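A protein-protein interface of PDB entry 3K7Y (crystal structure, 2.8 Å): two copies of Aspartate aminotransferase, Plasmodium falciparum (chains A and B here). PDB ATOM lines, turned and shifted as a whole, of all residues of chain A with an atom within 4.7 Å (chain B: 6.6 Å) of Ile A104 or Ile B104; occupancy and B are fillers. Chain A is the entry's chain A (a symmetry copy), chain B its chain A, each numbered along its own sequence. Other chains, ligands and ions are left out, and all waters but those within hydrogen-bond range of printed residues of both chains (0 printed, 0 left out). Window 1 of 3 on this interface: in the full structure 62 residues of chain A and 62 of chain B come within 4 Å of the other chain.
The backbone carbonyl oxygen of Tyr A286 sits at hydrogen-bond distance from the guanidinium group of Arg B257. The guanidinium group of Arg B257 is in hydrogen-bond range of the backbone carbonyl oxygen of Ser A288 (3.2 Å). The backbone carbonyl oxygen of Tyr B286 is in hydrogen-bond range of the guanidinium group of Arg A257. OG of Ser B287 lies within hydrogen-bond range of NH2 of Arg A257 (3.0 Å). O of Ser B288 sits at hydrogen-bond distance from NE of Arg A257. The backbone carbonyl oxygen (O) of Thr A107 lies close to the backbone carbonyl oxygen (O) of Phe B285, at 3.3 Å.
The backbone carbonyl oxygen (O) of Arg B257 is in hydrogen-bond range of the backbone NH (N) of Gly B105 (2.7 Å). The backbone NH (N) of Gly A105 is in hydrogen-bond range of the backbone carbonyl oxygen (O) of Arg A257, at 2.7 Å.
Of the printed residues of chain B, Ile A104 touches Ile B104 and Tyr B286. Of the printed residues of chain B, Thr A107 touches Phe B285 (3.1 Å), Tyr B286 (3.6 Å) and Ser B287 (3.8 Å). Of chain A, only Ile A104 and Tyr A286 come within 4 Å of Ile B104. Of the printed residues of chain A, Ser B288 touches Arg A257 (3.2 Å). Val B290 touches none of the printed residues of chain A. The nearest residue of chain B that does not touch Ile A104 is Ser B288 (4.3 Å).
Ile B104 touches its own counterpart, Ile A104. Ile A104 touches Tyr B286, and with the chains exchanged Tyr A286 touches Ile B104. Thr A107 touches Tyr B286, and with the chains exchanged Tyr A286 touches Thr B107. Arg A257 touches Tyr B286, and with the chains exchanged Tyr A286 touches Arg B257. Of the 14 pairs that touch across the chains among the printed residues, 9 have their exchanged pair printed and touching as well.
Hydrophobic or aromatic side chains of chain B that line the printed part of chain A: Ile B104 and Tyr B286. Among the printed residues, 14 pairs touch across the chains.
Among the printed residues, merely in contact across the chains: Thr A107 with Tyr B286 (3.6 Å), Tyr A286 with Thr B107 (3.6 Å), Tyr A286 with Ile B104 (3.7 Å), Ile A104 with Tyr B286 (3.7 Å), Ile A104 with Ile B104 (3.8 Å), Thr A107 with Ser B287 (3.8 Å), Arg A257 with Pro B289 (3.9 Å) and Gly A108 with Phe B285 (3.99 Å).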
ATOM      1  N   GLN A 102      24.695   2.752 -10.536  1.00  0.00           N
ATOM      2  CA  GLN A 102      23.709   2.942 -11.603  1.00  0.00           C
ATOM      3  C   GLN A 102      22.432   2.146 -11.299  1.00  0.00           C
ATOM      4  O   GLN A 102      22.499   0.937 -11.052  1.00  0.00           O
ATOM      5  CB  GLN A 102      24.282   2.507 -12.952  1.00  0.00           C
ATOM      6  CG  GLN A 102      23.276   2.561 -14.104  1.00  0.00           C
ATOM      7  CD  GLN A 102      23.824   2.005 -15.426  1.00  0.00           C
ATOM      8  OE1 GLN A 102      25.010   2.154 -15.740  1.00  0.00           O
ATOM      9  NE2 GLN A 102      22.954   1.365 -16.203  1.00  0.00           N
ATOM     10  N   CYS A 103      21.275   2.797 -11.325  1.00  0.00           N
ATOM     11  CA  CYS A 103      20.048   2.079 -11.043  1.00  0.00           C
ATOM     12  C   CYS A 103      19.075   2.135 -12.198  1.00  0.00           C
ATOM     13  O   CYS A 103      19.365   2.728 -13.240  1.00  0.00           O
ATOM     14  CB  CYS A 103      19.398   2.638  -9.796  1.00  0.00           C
ATOM     15  SG  CYS A 103      20.496   2.570  -8.394  1.00  0.00           S
ATOM     16  N   ILE A 104      17.908   1.535 -12.005  1.00  0.00           N
ATOM     17  CA  ILE A 104      16.889   1.514 -13.027  1.00  0.00           C
ATOM     18  C   ILE A 104      15.948   2.717 -12.825  1.00  0.00           C
ATOM     19  O   ILE A 104      14.828   2.599 -12.301  1.00  0.00           O
ATOM     20  CB  ILE A 104      16.203   0.148 -13.028  1.00  0.00           C
ATOM     21  CG1 ILE A 104      17.226  -0.885 -13.452  1.00  0.00           C
ATOM     22  CG2 ILE A 104      15.084   0.069 -14.021  1.00  0.00           C
ATOM     23  CD1 ILE A 104      17.081  -2.167 -12.695  1.00  0.00           C
ATOM     24  N   GLY A 105      16.435   3.885 -13.241  1.00  0.00           N
ATOM     25  CA  GLY A 105      15.689   5.120 -13.082  1.00  0.00           C
ATOM     26  C   GLY A 105      15.713   5.578 -11.639  1.00  0.00           C
ATOM     27  O   GLY A 105      16.350   4.932 -10.789  1.00  0.00           O
ATOM     28  N   GLY A 106      15.022   6.684 -11.355  1.00  0.00           N
ATOM     29  CA  GLY A 106      14.922   7.195  -9.989  1.00  0.00           C
ATOM     30  C   GLY A 106      14.258   6.204  -9.048  1.00  0.00           C
ATOM     31  O   GLY A 106      14.736   5.984  -7.938  1.00  0.00           O
ATOM     32  N   THR A 107      13.157   5.598  -9.511  1.00  0.00           N
ATOM     33  CA  THR A 107      12.430   4.519  -8.795  1.00  0.00           C
ATOM     34  C   THR A 107      13.410   3.445  -8.397  1.00  0.00           C
ATOM     35  O   THR A 107      13.425   2.986  -7.247  1.00  0.00           O
ATOM     36  CB  THR A 107      11.364   3.833  -9.711  1.00  0.00           C
ATOM     37  OG1 THR A 107      10.526   4.814 -10.324  1.00  0.00           O
ATOM     38  CG2 THR A 107      10.505   2.853  -8.940  1.00  0.00           C
ATOM     39  N   GLY A 108      14.228   3.048  -9.369  1.00  0.00           N
ATOM     40  CA  GLY A 108      15.198   2.008  -9.158  1.00  0.00           C
ATOM     41  C   GLY A 108      16.202   2.390  -8.097  1.00  0.00           C
ATOM     42  O   GLY A 108      16.734   1.532  -7.422  1.00  0.00           O
ATOM     43  N   ARG A 257      15.011   3.999 -18.495  1.00  0.00           N
ATOM     44  CA  ARG A 257      15.106   3.851 -17.037  1.00  0.00           C
ATOM     45  C   ARG A 257      16.482   4.249 -16.522  1.00  0.00           C
ATOM     46  O   ARG A 257      17.118   3.477 -15.795  1.00  0.00           O
ATOM     47  CB  ARG A 257      14.741   2.439 -16.582  1.00  0.00           C
ATOM     48  CG  ARG A 257      13.575   1.818 -17.327  1.00  0.00           C
ATOM     49  CD  ARG A 257      12.276   2.590 -17.141  1.00  0.00           C
ATOM     50  NE  ARG A 257      11.912   2.677 -15.731  1.00  0.00           N
ATOM     51  CZ  ARG A 257      12.016   3.773 -14.982  1.00  0.00           C
ATOM     52  NH1 ARG A 257      12.454   4.931 -15.502  1.00  0.00           N
ATOM     53  NH2 ARG A 257      11.666   3.707 -13.703  1.00  0.00           N
ATOM     54  N   GLY A 259      18.911   6.034 -14.057  1.00  0.00           N
ATOM     55  CA  GLY A 259      18.971   6.615 -12.712  1.00  0.00           C
ATOM     56  C   GLY A 259      20.254   6.317 -11.946  1.00  0.00           C
ATOM     57  O   GLY A 259      20.995   5.393 -12.289  1.00  0.00           O
ATOM     58  N   TYR A 286      18.176  -8.164  -9.469  1.00  0.00           N
ATOM     59  CA  TYR A 286      18.503  -8.241 -10.895  1.00  0.00           C
ATOM     60  C   TYR A 286      19.989  -8.357 -11.228  1.00  0.00           C
ATOM     61  O   TYR A 286      20.359  -8.213 -12.386  1.00  0.00           O
ATOM     62  CB  TYR A 286      17.918  -7.049 -11.643  1.00  0.00           C
ATOM     63  CG  TYR A 286      18.361  -5.705 -11.098  1.00  0.00           C
ATOM     64  CD1 TYR A 286      19.418  -4.992 -11.683  1.00  0.00           C
ATOM     65  CD2 TYR A 286      17.714  -5.138  -9.988  1.00  0.00           C
ATOM     66  CE1 TYR A 286      19.816  -3.758 -11.166  1.00  0.00           C
ATOM     67  CE2 TYR A 286      18.104  -3.914  -9.473  1.00  0.00           C
ATOM     68  CZ  TYR A 286      19.150  -3.230 -10.061  1.00  0.00           C
ATOM     69  OH  TYR A 286      19.526  -2.014  -9.540  1.00  0.00           O
ATOM     70  N   SER A 288      22.651  -6.989 -12.146  1.00  0.00           N
ATOM     71  CA  SER A 288      23.360  -5.803 -12.689  1.00  0.00           C
ATOM     72  C   SER A 288      22.529  -4.853 -13.573  1.00  0.00           C
ATOM     73  O   SER A 288      21.484  -5.245 -14.095  1.00  0.00           O
ATOM     74  CB  SER A 288      24.674  -6.197 -13.396  1.00  0.00           C
ATOM     75  OG  SER A 288      24.504  -7.242 -14.339  1.00  0.00           O
ATOM     76  N   GLN B 102       8.140  -8.410 -19.735  1.00  0.00           N
ATOM     77  CA  GLN B 102       9.569  -8.187 -19.967  1.00  0.00           C
ATOM     78  C   GLN B 102      10.288  -7.910 -18.641  1.00  0.00           C
ATOM     79  O   GLN B 102       9.881  -7.018 -17.887  1.00  0.00           O
ATOM     80  CB  GLN B 102       9.784  -7.018 -20.927  1.00  0.00           C
ATOM     81  CG  GLN B 102      11.253  -6.640 -21.133  1.00  0.00           C
ATOM     82  CD  GLN B 102      11.452  -5.389 -21.999  1.00  0.00           C
ATOM     83  OE1 GLN B 102      10.695  -5.137 -22.943  1.00  0.00           O
ATOM     84  NE2 GLN B 102      12.477  -4.604 -21.676  1.00  0.00           N
ATOM     85  N   CYS B 103      11.357  -8.646 -18.348  1.00  0.00           N
ATOM     86  CA  CYS B 103      12.062  -8.412 -17.104  1.00  0.00           C
ATOM     87  C   CYS B 103      13.506  -8.030 -17.331  1.00  0.00           C
ATOM     88  O   CYS B 103      13.960  -7.928 -18.472  1.00  0.00           O
ATOM     89  CB  CYS B 103      11.989  -9.646 -16.231  1.00  0.00           C
ATOM     90  SG  CYS B 103      10.302 -10.126 -15.909  1.00  0.00           S
ATOM     91  N   ILE B 104      14.235  -7.838 -16.238  1.00  0.00           N
ATOM     92  CA  ILE B 104      15.628  -7.469 -16.313  1.00  0.00           C
ATOM     93  C   ILE B 104      16.490  -8.744 -16.284  1.00  0.00           C
ATOM     94  O   ILE B 104      17.082  -9.120 -15.258  1.00  0.00           O
ATOM     95  CB  ILE B 104      15.940  -6.451 -15.217  1.00  0.00           C
ATOM     96  CG1 ILE B 104      15.167  -5.186 -15.522  1.00  0.00           C
ATOM     97  CG2 ILE B 104      17.388  -6.066 -15.185  1.00  0.00           C
ATOM     98  CD1 ILE B 104      14.630  -4.538 -14.285  1.00  0.00           C
ATOM     99  N   GLY B 105      16.539  -9.414 -17.435  1.00  0.00           N
ATOM    100  CA  GLY B 105      17.272 -10.660 -17.559  1.00  0.00           C
ATOM    101  C   GLY B 105      16.526 -11.792 -16.885  1.00  0.00           C
ATOM    102  O   GLY B 105      15.419 -11.583 -16.359  1.00  0.00           O
ATOM    103  N   GLY B 106      17.123 -12.986 -16.893  1.00  0.00           N
ATOM    104  CA  GLY B 106      16.528 -14.143 -16.227  1.00  0.00           C
ATOM    105  C   GLY B 106      16.361 -13.927 -14.732  1.00  0.00           C
ATOM    106  O   GLY B 106      15.314 -14.237 -14.172  1.00  0.00           O
ATOM    107  N   THR B 107      17.404 -13.376 -14.096  1.00  0.00           N
ATOM    108  CA  THR B 107      17.399 -12.979 -12.664  1.00  0.00           C
ATOM    109  C   THR B 107      16.191 -12.117 -12.397  1.00  0.00           C
ATOM    110  O   THR B 107      15.452 -12.333 -11.426  1.00  0.00           O
ATOM    111  CB  THR B 107      18.651 -12.119 -12.297  1.00  0.00           C
ATOM    112  OG1 THR B 107      19.847 -12.766 -12.734  1.00  0.00           O
ATOM    113  CG2 THR B 107      18.739 -11.858 -10.807  1.00  0.00           C
ATOM    114  N   GLY B 108      16.003 -11.132 -13.273  1.00  0.00           N
ATOM    115  CA  GLY B 108      14.916 -10.203 -13.137  1.00  0.00           C
ATOM    116  C   GLY B 108      13.577 -10.896 -13.219  1.00  0.00           C
ATOM    117  O   GLY B 108      12.615 -10.438 -12.634  1.00  0.00           O
ATOM    118  N   ALA B 109      13.491 -11.992 -13.954  1.00  0.00           N
ATOM    119  CA  ALA B 109      12.208 -12.650 -14.059  1.00  0.00           C
ATOM    120  C   ALA B 109      12.022 -13.577 -12.868  1.00  0.00           C
ATOM    121  O   ALA B 109      10.929 -13.669 -12.305  1.00  0.00           O
ATOM    122  CB  ALA B 109      12.078 -13.395 -15.368  1.00  0.00           C
ATOM    123  N   PHE B 111      13.194 -13.270  -9.820  1.00  0.00           N
ATOM    124  CA  PHE B 111      12.790 -12.506  -8.644  1.00  0.00           C
ATOM    125  C   PHE B 111      11.368 -11.954  -8.655  1.00  0.00           C
ATOM    126  O   PHE B 111      10.719 -12.060  -7.630  1.00  0.00           O
ATOM    127  CB  PHE B 111      13.799 -11.431  -8.285  1.00  0.00           C
ATOM    128  CG  PHE B 111      13.380 -10.059  -8.628  1.00  0.00           C
ATOM    129  CD1 PHE B 111      14.057  -9.354  -9.602  1.00  0.00           C
ATOM    130  CD2 PHE B 111      12.341  -9.439  -7.932  1.00  0.00           C
ATOM    131  CE1 PHE B 111      13.701  -8.036  -9.895  1.00  0.00           C
ATOM    132  CE2 PHE B 111      11.969  -8.141  -8.209  1.00  0.00           C
ATOM    133  CZ  PHE B 111      12.647  -7.431  -9.196  1.00  0.00           C
ATOM    134  N   GLU B 256      22.762  -6.113 -21.410  1.00  0.00           N
ATOM    135  CA  GLU B 256      21.481  -5.534 -21.785  1.00  0.00           C
ATOM    136  C   GLU B 256      20.390  -5.927 -20.789  1.00  0.00           C
ATOM    137  O   GLU B 256      19.359  -5.253 -20.664  1.00  0.00           O
ATOM    138  CB  GLU B 256      21.113  -5.980 -23.195  1.00  0.00           C
ATOM    139  CG  GLU B 256      21.315  -4.959 -24.326  1.00  0.00           C
ATOM    140  CD  GLU B 256      22.168  -3.747 -23.960  1.00  0.00           C
ATOM    141  OE1 GLU B 256      21.697  -2.878 -23.186  1.00  0.00           O
ATOM    142  OE2 GLU B 256      23.291  -3.643 -24.494  1.00  0.00           O
ATOM    143  N   ARG B 257      20.655  -7.019 -20.073  1.00  0.00           N
ATOM    144  CA  ARG B 257      19.734  -7.640 -19.112  1.00  0.00           C
ATOM    145  C   ARG B 257      18.404  -7.996 -19.760  1.00  0.00           C
ATOM    146  O   ARG B 257      17.344  -7.618 -19.247  1.00  0.00           O
ATOM    147  CB  ARG B 257      19.523  -6.766 -17.878  1.00  0.00           C
ATOM    148  CG  ARG B 257      20.773  -6.066 -17.378  1.00  0.00           C
ATOM    149  CD  ARG B 257      21.856  -7.039 -16.933  1.00  0.00           C
ATOM    150  NE  ARG B 257      21.376  -7.913 -15.869  1.00  0.00           N
ATOM    151  CZ  ARG B 257      21.067  -9.200 -16.018  1.00  0.00           C
ATOM    152  NH1 ARG B 257      21.212  -9.816 -17.203  1.00  0.00           N
ATOM    153  NH2 ARG B 257      20.622  -9.875 -14.966  1.00  0.00           N
ATOM    154  N   ALA B 258      18.446  -8.720 -20.884  1.00  0.00           N
ATOM    155  CA  ALA B 258      17.200  -9.127 -21.568  1.00  0.00           C
ATOM    156  C   ALA B 258      16.609 -10.425 -20.979  1.00  0.00           C
ATOM    157  O   ALA B 258      17.283 -11.479 -20.968  1.00  0.00           O
ATOM    158  CB  ALA B 258      17.417  -9.263 -23.072  1.00  0.00           C
ATOM    159  N   GLY B 259      15.376 -10.339 -20.470  1.00  0.00           N
ATOM    160  CA  GLY B 259      14.676 -11.515 -19.943  1.00  0.00           C
ATOM    161  C   GLY B 259      13.157 -11.439 -20.014  1.00  0.00           C
ATOM    162  O   GLY B 259      12.585 -10.357 -20.168  1.00  0.00           O
ATOM    163  N   ALA B 260      12.494 -12.583 -19.875  1.00  0.00           N
ATOM    164  CA  ALA B 260      11.041 -12.623 -19.877  1.00  0.00           C
ATOM    165  C   ALA B 260      10.482 -13.562 -18.802  1.00  0.00           C
ATOM    166  O   ALA B 260      11.197 -14.419 -18.307  1.00  0.00           O
ATOM    167  CB  ALA B 260      10.555 -13.023 -21.240  1.00  0.00           C
ATOM    168  N   PHE B 285       9.158  -1.567  -7.074  1.00  0.00           N
ATOM    169  CA  PHE B 285      10.569  -1.792  -7.371  1.00  0.00           C
ATOM    170  C   PHE B 285      11.133  -0.796  -8.405  1.00  0.00           C
ATOM    171  O   PHE B 285      11.798   0.183  -8.028  1.00  0.00           O
ATOM    172  CB  PHE B 285      10.820  -3.265  -7.759  1.00  0.00           C
ATOM    173  CG  PHE B 285      10.624  -4.225  -6.616  1.00  0.00           C
ATOM    174  CD1 PHE B 285      11.564  -4.308  -5.583  1.00  0.00           C
ATOM    175  CD2 PHE B 285       9.486  -5.013  -6.536  1.00  0.00           C
ATOM    176  CE1 PHE B 285      11.367  -5.170  -4.487  1.00  0.00           C
ATOM    177  CE2 PHE B 285       9.285  -5.876  -5.451  1.00  0.00           C
ATOM    178  CZ  PHE B 285      10.234  -5.950  -4.427  1.00  0.00           C
ATOM    179  N   TYR B 286      10.868  -1.027  -9.693  1.00  0.00           N
ATOM    180  CA  TYR B 286      11.389  -0.159 -10.754  1.00  0.00           C
ATOM    181  C   TYR B 286      10.353   0.376 -11.739  1.00  0.00           C
ATOM    182  O   TYR B 286      10.729   0.926 -12.765  1.00  0.00           O
ATOM    183  CB  TYR B 286      12.494  -0.867 -11.528  1.00  0.00           C
ATOM    184  CG  TYR B 286      12.070  -2.193 -12.128  1.00  0.00           C
ATOM    185  CD1 TYR B 286      11.671  -2.295 -13.469  1.00  0.00           C
ATOM    186  CD2 TYR B 286      12.071  -3.361 -11.349  1.00  0.00           C
ATOM    187  CE1 TYR B 286      11.278  -3.523 -14.004  1.00  0.00           C
ATOM    188  CE2 TYR B 286      11.686  -4.582 -11.876  1.00  0.00           C
ATOM    189  CZ  TYR B 286      11.292  -4.658 -13.198  1.00  0.00           C
ATOM    190  OH  TYR B 286      10.912  -5.877 -13.708  1.00  0.00           O
ATOM    191  N   SER B 287       9.066   0.200 -11.445  1.00  0.00           N
ATOM    192  CA  SER B 287       7.963   0.689 -12.288  1.00  0.00           C
ATOM    193  C   SER B 287       7.873   0.180 -13.757  1.00  0.00           C
ATOM    194  O   SER B 287       6.790  -0.224 -14.177  1.00  0.00           O
ATOM    195  CB  SER B 287       7.878   2.204 -12.220  1.00  0.00           C
ATOM    196  OG  SER B 287       8.844   2.783 -13.077  1.00  0.00           O
ATOM    197  N   SER B 288       8.959   0.189 -14.536  1.00  0.00           N
ATOM    198  CA  SER B 288       8.902  -0.390 -15.901  1.00  0.00           C
ATOM    199  C   SER B 288      10.238  -0.868 -16.501  1.00  0.00           C
ATOM    200  O   SER B 288      11.306  -0.455 -16.045  1.00  0.00           O
ATOM    201  CB  SER B 288       8.165   0.543 -16.886  1.00  0.00           C
ATOM    202  OG  SER B 288       8.645   1.876 -16.852  1.00  0.00           O
ATOM    203  N   PRO B 289      10.178  -1.739 -17.539  1.00  0.00           N
ATOM    204  CA  PRO B 289      11.356  -2.297 -18.208  1.00  0.00           C
ATOM    205  C   PRO B 289      12.017  -1.351 -19.205  1.00  0.00           C
ATOM    206  O   PRO B 289      11.400  -0.368 -19.651  1.00  0.00           O
ATOM    207  CB  PRO B 289      10.785  -3.490 -18.983  1.00  0.00           C
ATOM    208  CG  PRO B 289       9.383  -3.666 -18.489  1.00  0.00           C
ATOM    209  CD  PRO B 289       8.945  -2.310 -18.104  1.00  0.00           C
ATOM    210  N   VAL B 290      13.266  -1.674 -19.556  1.00  0.00           N
ATOM    211  CA  VAL B 290      14.067  -0.933 -20.545  1.00  0.00           C
ATOM    212  C   VAL B 290      13.509  -1.030 -21.975  1.00  0.00           C
ATOM    213  O   VAL B 290      13.291  -2.125 -22.521  1.00  0.00           O
ATOM    214  CB  VAL B 290      15.559  -1.346 -20.488  1.00  0.00           C
ATOM    215  CG1 VAL B 290      16.391  -0.630 -21.570  1.00  0.00           C
ATOM    216  CG2 VAL B 290      16.104  -1.050 -19.108  1.00  0.00           C
